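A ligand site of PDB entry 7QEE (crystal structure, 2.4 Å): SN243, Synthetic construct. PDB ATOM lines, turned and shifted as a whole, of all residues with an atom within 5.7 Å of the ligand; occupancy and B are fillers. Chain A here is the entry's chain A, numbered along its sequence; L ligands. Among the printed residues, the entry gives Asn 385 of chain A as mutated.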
ATOM      1  N   VAL A 104     -18.301 -15.294  32.073  1.00  0.00           N
ATOM      2  CA  VAL A 104     -18.792 -14.612  30.878  1.00  0.00           C
ATOM      3  C   VAL A 104     -20.267 -14.938  30.712  1.00  0.00           C
ATOM      4  O   VAL A 104     -20.643 -16.102  30.510  1.00  0.00           O
ATOM      5  CB  VAL A 104     -18.024 -15.004  29.618  1.00  0.00           C
ATOM      6  CG1 VAL A 104     -18.595 -14.223  28.441  1.00  0.00           C
ATOM      7  CG2 VAL A 104     -16.525 -14.740  29.780  1.00  0.00           C
ATOM      8  N   ARG A 106     -23.447 -14.853  28.469  1.00  0.00           N
ATOM      9  CA  ARG A 106     -23.646 -14.839  27.023  1.00  0.00           C
ATOM     10  C   ARG A 106     -25.095 -14.934  26.541  1.00  0.00           C
ATOM     11  O   ARG A 106     -25.316 -14.939  25.319  1.00  0.00           O
ATOM     12  CB  ARG A 106     -22.852 -15.969  26.378  1.00  0.00           C
ATOM     13  CG  ARG A 106     -21.446 -16.015  26.842  1.00  0.00           C
ATOM     14  CD  ARG A 106     -20.688 -16.989  25.980  1.00  0.00           C
ATOM     15  NE  ARG A 106     -19.278 -16.976  26.301  1.00  0.00           N
ATOM     16  CZ  ARG A 106     -18.410 -16.106  25.816  1.00  0.00           C
ATOM     17  NH1 ARG A 106     -18.808 -15.176  24.957  1.00  0.00           N
ATOM     18  NH2 ARG A 106     -17.150 -16.181  26.187  1.00  0.00           N
ATOM     19  N   ASN A 156     -19.491  -9.819  25.917  1.00  0.00           N
ATOM     20  CA  ASN A 156     -19.290  -9.078  24.702  1.00  0.00           C
ATOM     21  C   ASN A 156     -20.386  -8.020  24.561  1.00  0.00           C
ATOM     22  O   ASN A 156     -21.320  -7.938  25.367  1.00  0.00           O
ATOM     23  CB  ASN A 156     -19.185 -10.066  23.533  1.00  0.00           C
ATOM     24  CG  ASN A 156     -17.842 -10.841  23.551  1.00  0.00           C
ATOM     25  OD1 ASN A 156     -16.776 -10.256  23.694  1.00  0.00           O
ATOM     26  ND2 ASN A 156     -17.910 -12.160  23.407  1.00  0.00           N
ATOM     27  N   TYR A 228     -15.835  -7.810  28.166  1.00  0.00           N
ATOM     28  CA  TYR A 228     -14.830  -8.250  27.199  1.00  0.00           C
ATOM     29  C   TYR A 228     -14.882  -7.241  26.051  1.00  0.00           C
ATOM     30  O   TYR A 228     -15.577  -7.423  25.048  1.00  0.00           O
ATOM     31  CB  TYR A 228     -15.133  -9.649  26.693  1.00  0.00           C
ATOM     32  CG  TYR A 228     -14.506 -10.763  27.498  1.00  0.00           C
ATOM     33  CD1 TYR A 228     -13.836 -10.510  28.701  1.00  0.00           C
ATOM     34  CD2 TYR A 228     -14.553 -12.073  27.050  1.00  0.00           C
ATOM     35  CE1 TYR A 228     -13.256 -11.529  29.412  1.00  0.00           C
ATOM     36  CE2 TYR A 228     -13.976 -13.096  27.748  1.00  0.00           C
ATOM     37  CZ  TYR A 228     -13.325 -12.825  28.933  1.00  0.00           C
ATOM     38  OH  TYR A 228     -12.769 -13.884  29.617  1.00  0.00           O
ATOM     39  N   TYR A 241     -11.786  -9.495   8.817  1.00  0.00           N
ATOM     40  CA  TYR A 241     -13.226  -9.633   9.027  1.00  0.00           C
ATOM     41  C   TYR A 241     -13.703  -8.894  10.277  1.00  0.00           C
ATOM     42  O   TYR A 241     -14.832  -8.421  10.319  1.00  0.00           O
ATOM     43  CB  TYR A 241     -13.637 -11.109   9.086  1.00  0.00           C
ATOM     44  CG  TYR A 241     -13.479 -11.792  10.442  1.00  0.00           C
ATOM     45  CD1 TYR A 241     -14.443 -11.680  11.434  1.00  0.00           C
ATOM     46  CD2 TYR A 241     -12.359 -12.547  10.708  1.00  0.00           C
ATOM     47  CE1 TYR A 241     -14.271 -12.310  12.662  1.00  0.00           C
ATOM     48  CE2 TYR A 241     -12.181 -13.193  11.925  1.00  0.00           C
ATOM     49  CZ  TYR A 241     -13.127 -13.063  12.900  1.00  0.00           C
ATOM     50  OH  TYR A 241     -12.917 -13.689  14.104  1.00  0.00           O
ATOM     51  N   ARG A 242     -12.854  -8.664  11.272  1.00  0.00           N
ATOM     52  CA  ARG A 242     -13.306  -8.053  12.541  1.00  0.00           C
ATOM     53  C   ARG A 242     -13.513  -6.534  12.444  1.00  0.00           C
ATOM     54  O   ARG A 242     -13.953  -5.951  13.423  1.00  0.00           O
ATOM     55  CB  ARG A 242     -12.360  -8.468  13.671  1.00  0.00           C
ATOM     56  CG  ARG A 242     -12.368  -9.956  13.964  1.00  0.00           C
ATOM     57  CD  ARG A 242     -11.865 -10.313  15.353  1.00  0.00           C
ATOM     58  NE  ARG A 242     -12.810 -10.004  16.417  1.00  0.00           N
ATOM     59  CZ  ARG A 242     -12.674 -10.379  17.675  1.00  0.00           C
ATOM     60  NH1 ARG A 242     -11.620 -11.079  18.048  1.00  0.00           N
ATOM     61  NH2 ARG A 242     -13.594 -10.046  18.565  1.00  0.00           N
ATOM     62  N   HIS A 244     -15.819  -5.156  11.605  1.00  0.00           N
ATOM     63  CA  HIS A 244     -17.240  -4.927  11.933  1.00  0.00           C
ATOM     64  C   HIS A 244     -17.404  -4.459  13.381  1.00  0.00           C
ATOM     65  O   HIS A 244     -18.420  -3.869  13.665  1.00  0.00           O
ATOM     66  CB  HIS A 244     -18.046  -6.175  11.588  1.00  0.00           C
ATOM     67  CG  HIS A 244     -18.010  -7.283  12.577  1.00  0.00           C
ATOM     68  ND1 HIS A 244     -18.779  -7.280  13.724  1.00  0.00           N
ATOM     69  CD2 HIS A 244     -17.357  -8.471  12.565  1.00  0.00           C
ATOM     70  CE1 HIS A 244     -18.572  -8.390  14.392  1.00  0.00           C
ATOM     71  NE2 HIS A 244     -17.712  -9.138  13.698  1.00  0.00           N
ATOM     72  N   GLU A 245     -16.384  -4.664  14.217  1.00  0.00           N
ATOM     73  CA  GLU A 245     -16.449  -4.271  15.643  1.00  0.00           C
ATOM     74  C   GLU A 245     -15.383  -3.210  15.937  1.00  0.00           C
ATOM     75  O   GLU A 245     -15.083  -3.011  17.099  1.00  0.00           O
ATOM     76  CB  GLU A 245     -16.292  -5.501  16.523  1.00  0.00           C
ATOM     77  CG  GLU A 245     -15.895  -6.747  15.765  1.00  0.00           C
ATOM     78  CD  GLU A 245     -15.919  -8.009  16.613  1.00  0.00           C
ATOM     79  OE1 GLU A 245     -16.223  -7.899  17.811  1.00  0.00           O
ATOM     80  OE2 GLU A 245     -15.642  -9.080  16.073  1.00  0.00           O
ATOM     81  N   LYS A 288      -9.394  -4.609  24.540  1.00  0.00           N
ATOM     82  CA  LYS A 288      -8.878  -5.661  23.667  1.00  0.00           C
ATOM     83  C   LYS A 288      -8.697  -5.078  22.284  1.00  0.00           C
ATOM     84  O   LYS A 288      -9.251  -4.011  21.985  1.00  0.00           O
ATOM     85  CB  LYS A 288      -9.858  -6.850  23.631  1.00  0.00           C
ATOM     86  CG  LYS A 288     -11.246  -6.544  23.087  1.00  0.00           C
ATOM     87  CD  LYS A 288     -12.197  -7.763  23.262  1.00  0.00           C
ATOM     88  CE  LYS A 288     -13.556  -7.554  22.579  1.00  0.00           C
ATOM     89  NZ  LYS A 288     -14.495  -8.719  22.680  1.00  0.00           N
ATOM     90  N   HIS A 289      -7.918  -5.760  21.429  1.00  0.00           N
ATOM     91  CA  HIS A 289      -7.009  -6.861  21.781  1.00  0.00           C
ATOM     92  C   HIS A 289      -5.539  -6.369  21.791  1.00  0.00           C
ATOM     93  O   HIS A 289      -4.929  -6.139  20.735  1.00  0.00           O
ATOM     94  CB  HIS A 289      -7.153  -8.020  20.810  1.00  0.00           C
ATOM     95  CG  HIS A 289      -8.559  -8.519  20.639  1.00  0.00           C
ATOM     96  ND1 HIS A 289      -9.403  -8.081  19.642  1.00  0.00           N
ATOM     97  CD2 HIS A 289      -9.266  -9.434  21.354  1.00  0.00           C
ATOM     98  CE1 HIS A 289     -10.568  -8.710  19.739  1.00  0.00           C
ATOM     99  NE2 HIS A 289     -10.505  -9.534  20.766  1.00  0.00           N
ATOM    100  N   HIS A 303      -7.467 -16.301  14.995  1.00  0.00           N
ATOM    101  CA  HIS A 303      -8.278 -17.432  15.433  1.00  0.00           C
ATOM    102  C   HIS A 303      -7.873 -18.692  14.700  1.00  0.00           C
ATOM    103  O   HIS A 303      -8.038 -19.801  15.224  1.00  0.00           O
ATOM    104  CB  HIS A 303      -9.760 -17.190  15.142  1.00  0.00           C
ATOM    105  CG  HIS A 303     -10.441 -16.392  16.196  1.00  0.00           C
ATOM    106  ND1 HIS A 303     -10.383 -15.023  16.240  1.00  0.00           N
ATOM    107  CD2 HIS A 303     -11.152 -16.787  17.276  1.00  0.00           C
ATOM    108  CE1 HIS A 303     -11.055 -14.599  17.296  1.00  0.00           C
ATOM    109  NE2 HIS A 303     -11.520 -15.647  17.945  1.00  0.00           N
ATOM    110  N   MET A 336      -6.931  -7.442  27.442  1.00  0.00           N
ATOM    111  CA  MET A 336      -6.864  -8.730  26.760  1.00  0.00           C
ATOM    112  C   MET A 336      -5.828  -8.691  25.655  1.00  0.00           C
ATOM    113  O   MET A 336      -6.008  -7.938  24.689  1.00  0.00           O
ATOM    114  CB  MET A 336      -8.242  -9.077  26.186  1.00  0.00           C
ATOM    115  CG  MET A 336      -8.373 -10.521  25.725  1.00  0.00           C
ATOM    116  SD  MET A 336     -10.000 -10.986  25.065  1.00  0.00           S
ATOM    117  CE  MET A 336     -10.960 -11.115  26.554  1.00  0.00           C
ATOM    118  N   TYR A 338      -4.033 -10.180  22.224  1.00  0.00           N
ATOM    119  CA  TYR A 338      -4.589 -10.928  21.092  1.00  0.00           C
ATOM    120  C   TYR A 338      -3.848 -12.245  20.851  1.00  0.00           C
ATOM    121  O   TYR A 338      -2.862 -12.581  21.526  1.00  0.00           O
ATOM    122  CB  TYR A 338      -4.594 -10.101  19.810  1.00  0.00           C
ATOM    123  CG  TYR A 338      -5.720 -10.523  18.881  1.00  0.00           C
ATOM    124  CD1 TYR A 338      -6.914 -11.008  19.404  1.00  0.00           C
ATOM    125  CD2 TYR A 338      -5.584 -10.484  17.501  1.00  0.00           C
ATOM    126  CE1 TYR A 338      -7.932 -11.423  18.598  1.00  0.00           C
ATOM    127  CE2 TYR A 338      -6.629 -10.886  16.680  1.00  0.00           C
ATOM    128  CZ  TYR A 338      -7.799 -11.362  17.241  1.00  0.00           C
ATOM    129  OH  TYR A 338      -8.858 -11.790  16.470  1.00  0.00           O
ATOM    130  N   TYR A 339      -4.325 -13.000  19.867  1.00  0.00           N
ATOM    131  CA  TYR A 339      -3.672 -14.257  19.506  1.00  0.00           C
ATOM    132  C   TYR A 339      -2.543 -14.056  18.510  1.00  0.00           C
ATOM    133  O   TYR A 339      -1.723 -14.955  18.342  1.00  0.00           O
ATOM    134  CB  TYR A 339      -4.640 -15.226  18.827  1.00  0.00           C
ATOM    135  CG  TYR A 339      -5.995 -15.495  19.410  1.00  0.00           C
ATOM    136  CD1 TYR A 339      -6.147 -16.248  20.574  1.00  0.00           C
ATOM    137  CD2 TYR A 339      -7.138 -15.083  18.744  1.00  0.00           C
ATOM    138  CE1 TYR A 339      -7.409 -16.540  21.071  1.00  0.00           C
ATOM    139  CE2 TYR A 339      -8.395 -15.358  19.220  1.00  0.00           C
ATOM    140  CZ  TYR A 339      -8.536 -16.085  20.388  1.00  0.00           C
ATOM    141  OH  TYR A 339      -9.804 -16.357  20.872  1.00  0.00           O
ATOM    142  N   ASN A 385      -7.202 -13.955  26.072  1.00  0.00           N
ATOM    143  CA  ASN A 385      -8.262 -14.303  25.143  1.00  0.00           C
ATOM    144  C   ASN A 385      -8.664 -15.771  25.328  1.00  0.00           C
ATOM    145  O   ASN A 385      -7.991 -16.548  26.027  1.00  0.00           O
ATOM    146  CB  ASN A 385      -7.842 -14.008  23.719  1.00  0.00           C
ATOM    147  CG  ASN A 385      -9.033 -13.738  22.808  1.00  0.00           C
ATOM    148  OD1 ASN A 385     -10.170 -14.042  23.165  1.00  0.00           O
ATOM    149  ND2 ASN A 385      -8.778 -13.120  21.658  1.00  0.00           N
ATOM    150  N   THR A 386      -9.768 -16.172  24.700  1.00  0.00           N
ATOM    151  CA  THR A 386     -10.396 -17.452  24.989  1.00  0.00           C
ATOM    152  C   THR A 386      -9.902 -18.574  24.077  1.00  0.00           C
ATOM    153  O   THR A 386      -9.969 -18.470  22.849  1.00  0.00           O
ATOM    154  CB  THR A 386     -11.903 -17.309  24.852  1.00  0.00           C
ATOM    155  OG1 THR A 386     -12.320 -16.177  25.602  1.00  0.00           O
ATOM    156  CG2 THR A 386     -12.589 -18.546  25.403  1.00  0.00           C
ATOM    157  N   SER A 417      -9.192 -17.305  29.969  1.00  0.00           N
ATOM    158  CA  SER A 417     -10.567 -17.378  29.549  1.00  0.00           C
ATOM    159  C   SER A 417     -10.779 -18.689  28.790  1.00  0.00           C
ATOM    160  O   SER A 417      -9.982 -19.037  27.912  1.00  0.00           O
ATOM    161  CB  SER A 417     -10.906 -16.168  28.680  1.00  0.00           C
ATOM    162  OG  SER A 417     -12.093 -16.348  27.883  1.00  0.00           O
ATOM    163  N   ARG A 621     -15.847 -20.829  11.896  1.00  0.00           N
ATOM    164  CA  ARG A 621     -17.004 -20.493  12.730  1.00  0.00           C
ATOM    165  C   ARG A 621     -17.000 -19.044  13.190  1.00  0.00           C
ATOM    166  O   ARG A 621     -18.074 -18.467  13.406  1.00  0.00           O
ATOM    167  CB  ARG A 621     -17.076 -21.429  13.929  1.00  0.00           C
ATOM    168  CG  ARG A 621     -15.800 -21.563  14.738  1.00  0.00           C
ATOM    169  CD  ARG A 621     -15.942 -22.717  15.737  1.00  0.00           C
ATOM    170  NE  ARG A 621     -14.716 -23.035  16.476  1.00  0.00           N
ATOM    171  CZ  ARG A 621     -13.842 -23.980  16.124  1.00  0.00           C
ATOM    172  NH1 ARG A 621     -12.751 -24.200  16.868  1.00  0.00           N
ATOM    173  NH2 ARG A 621     -14.056 -24.714  15.023  1.00  0.00           N
ATOM    174  N   PHE A 622     -15.829 -18.430  13.364  1.00  0.00           N
ATOM    175  CA  PHE A 622     -15.817 -17.101  13.934  1.00  0.00           C
ATOM    176  C   PHE A 622     -16.043 -16.025  12.893  1.00  0.00           C
ATOM    177  O   PHE A 622     -16.289 -14.872  13.268  1.00  0.00           O
ATOM    178  CB  PHE A 622     -14.510 -16.842  14.658  1.00  0.00           C
ATOM    179  CG  PHE A 622     -14.189 -17.848  15.702  1.00  0.00           C
ATOM    180  CD1 PHE A 622     -14.853 -17.852  16.916  1.00  0.00           C
ATOM    181  CD2 PHE A 622     -13.212 -18.816  15.476  1.00  0.00           C
ATOM    182  CE1 PHE A 622     -14.545 -18.788  17.884  1.00  0.00           C
ATOM    183  CE2 PHE A 622     -12.907 -19.756  16.431  1.00  0.00           C
ATOM    184  CZ  PHE A 622     -13.571 -19.743  17.639  1.00  0.00           C
ATOM    185  N   GLY A 623     -15.935 -16.374  11.611  1.00  0.00           N
ATOM    186  CA  GLY A 623     -16.052 -15.414  10.537  1.00  0.00           C
ATOM    187  C   GLY A 623     -14.842 -15.428   9.625  1.00  0.00           C
ATOM    188  O   GLY A 623     -13.845 -16.117   9.875  1.00  0.00           O
HETATM  189  C1  LIG L   1     -14.956 -14.307  24.223  1.00  0.00           C
HETATM  190  C2  LIG L   1     -15.165 -15.565  19.544  1.00  0.00           C
HETATM  191  C3  LIG L   1     -16.083 -14.371  17.691  1.00  0.00           C
HETATM  192  C4  LIG L   1     -12.603 -12.067  22.077  1.00  0.00           C
HETATM  193  C5  LIG L   1     -12.394 -13.047  20.931  1.00  0.00           C
HETATM  194  C6  LIG L   1     -12.658 -14.490  21.341  1.00  0.00           C
HETATM  195  C7  LIG L   1     -13.802 -13.834  23.339  1.00  0.00           C
HETATM  196  C8  LIG L   1     -13.858 -12.377  22.870  1.00  0.00           C
HETATM  197  C9  LIG L   1     -13.956 -14.920  19.335  1.00  0.00           C
HETATM  198  C10 LIG L   1     -16.245 -15.292  18.726  1.00  0.00           C
HETATM  199  C11 LIG L   1     -14.882 -13.741  17.442  1.00  0.00           C
HETATM  200  C12 LIG L   1     -13.821 -14.032  18.278  1.00  0.00           C
HETATM  201  N1  LIG L   1     -17.192 -14.083  16.797  1.00  0.00           N
HETATM  202  O1  LIG L   1     -12.688 -10.755  21.529  1.00  0.00           O
HETATM  203  O2  LIG L   1     -11.099 -12.933  20.361  1.00  0.00           O
HETATM  204  O3  LIG L   1     -13.800 -14.658  22.168  1.00  0.00           O
HETATM  205  O4  LIG L   1     -13.957 -11.475  23.985  1.00  0.00           O
HETATM  206  O5  LIG L   1     -16.079 -13.874  24.065  1.00  0.00           O
HETATM  207  O6  LIG L   1     -14.725 -15.138  25.070  1.00  0.00           O
HETATM  208  O7  LIG L   1     -12.854 -15.215  20.142  1.00  0.00           O
HETATM  209  O8  LIG L   1     -17.105 -13.091  16.086  1.00  0.00           O
HETATM  210  O9  LIG L   1     -18.136 -14.861  16.745  1.00  0.00           O
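The guanidinium group (NH1) of Arg 242 is in hydrogen-bond range of an oxygen (O2) of the ligand. NZ of Lys 288 sits at hydrogen-bond distance from O1 of the ligand (3.0 Å). OG1 of Thr 386 lies within hydrogen-bond range of O6 of the ligand, 2.7 Å away. The guanidinium group (NH2) of Arg 106 lies within salt-bridge range of an oxygen (O6) of the ligand (2.9 Å). The side-chain amide nitrogen (ND2) of Asn 156 sits at hydrogen-bond distance from an oxygen (O5) of the ligand. An oxygen (O2) of the ligand sits at hydrogen-bond distance from the side-chain amide nitrogen (ND2) of Asn 385 (2.7 Å). A ring nitrogen (NE2) of His 303 is in hydrogen-bond range of an oxygen (O7) of the ligand, 2.6 Å away. OH of Tyr 339 lies within hydrogen-bond range of O7 of the ligand (3.3 Å). A ring nitrogen (NE2) of His 289 lies within hydrogen-bond range of an oxygen (O1) of the ligand (2.6 Å).
A ring nitrogen (NE2) of His 289 lies close to the guanidinium group of Arg 242, at 3.3 Å. The side-chain amide oxygen (OD1) of Asn 385 lies within hydrogen-bond range of the side-chain hydroxyl (OH) of Tyr 339 (3.3 Å). OG of Ser 417 lies within hydrogen-bond range of OH of Tyr 228 (3.1 Å). The side-chain amide oxygen (OD1) of Asn 156 sits close to the backbone carbonyl oxygen (O) of Tyr 228 (3.4 Å). A ring nitrogen (NE2) of His 303 lies close to the side-chain hydroxyl (OH) of Tyr 339, at 3.5 Å. The guanidinium group (NE) of Arg 242 is in salt-bridge range of the side-chain carboxylate (OE2) of Glu 245. OH of Tyr 338 lies within hydrogen-bond range of NH1 of Arg 242. The side-chain sulfur of Met 336 lies close to the side-chain amide oxygen of Asn 385 (3.6 Å).
O8 of the ligand sits close to O of Phe 622 (3.4 Å). Tyr 228 touches the ligand. Tyr 241 touches the ligand (OH to C11, 3.9 Å). CE of Met 336 touches O4 of the ligand, at 3.96 Å. CE1 of Tyr 338 touches O2 of the ligand (3.9 Å). Within 4 Å of the ligand: Arg 106, Asn 156, Tyr 228, Tyr 241, Arg 242, Lys 288, His 289, His 303, Met 336, Tyr 338, Tyr 339, Asn 385, Thr 386 and Phe 622.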
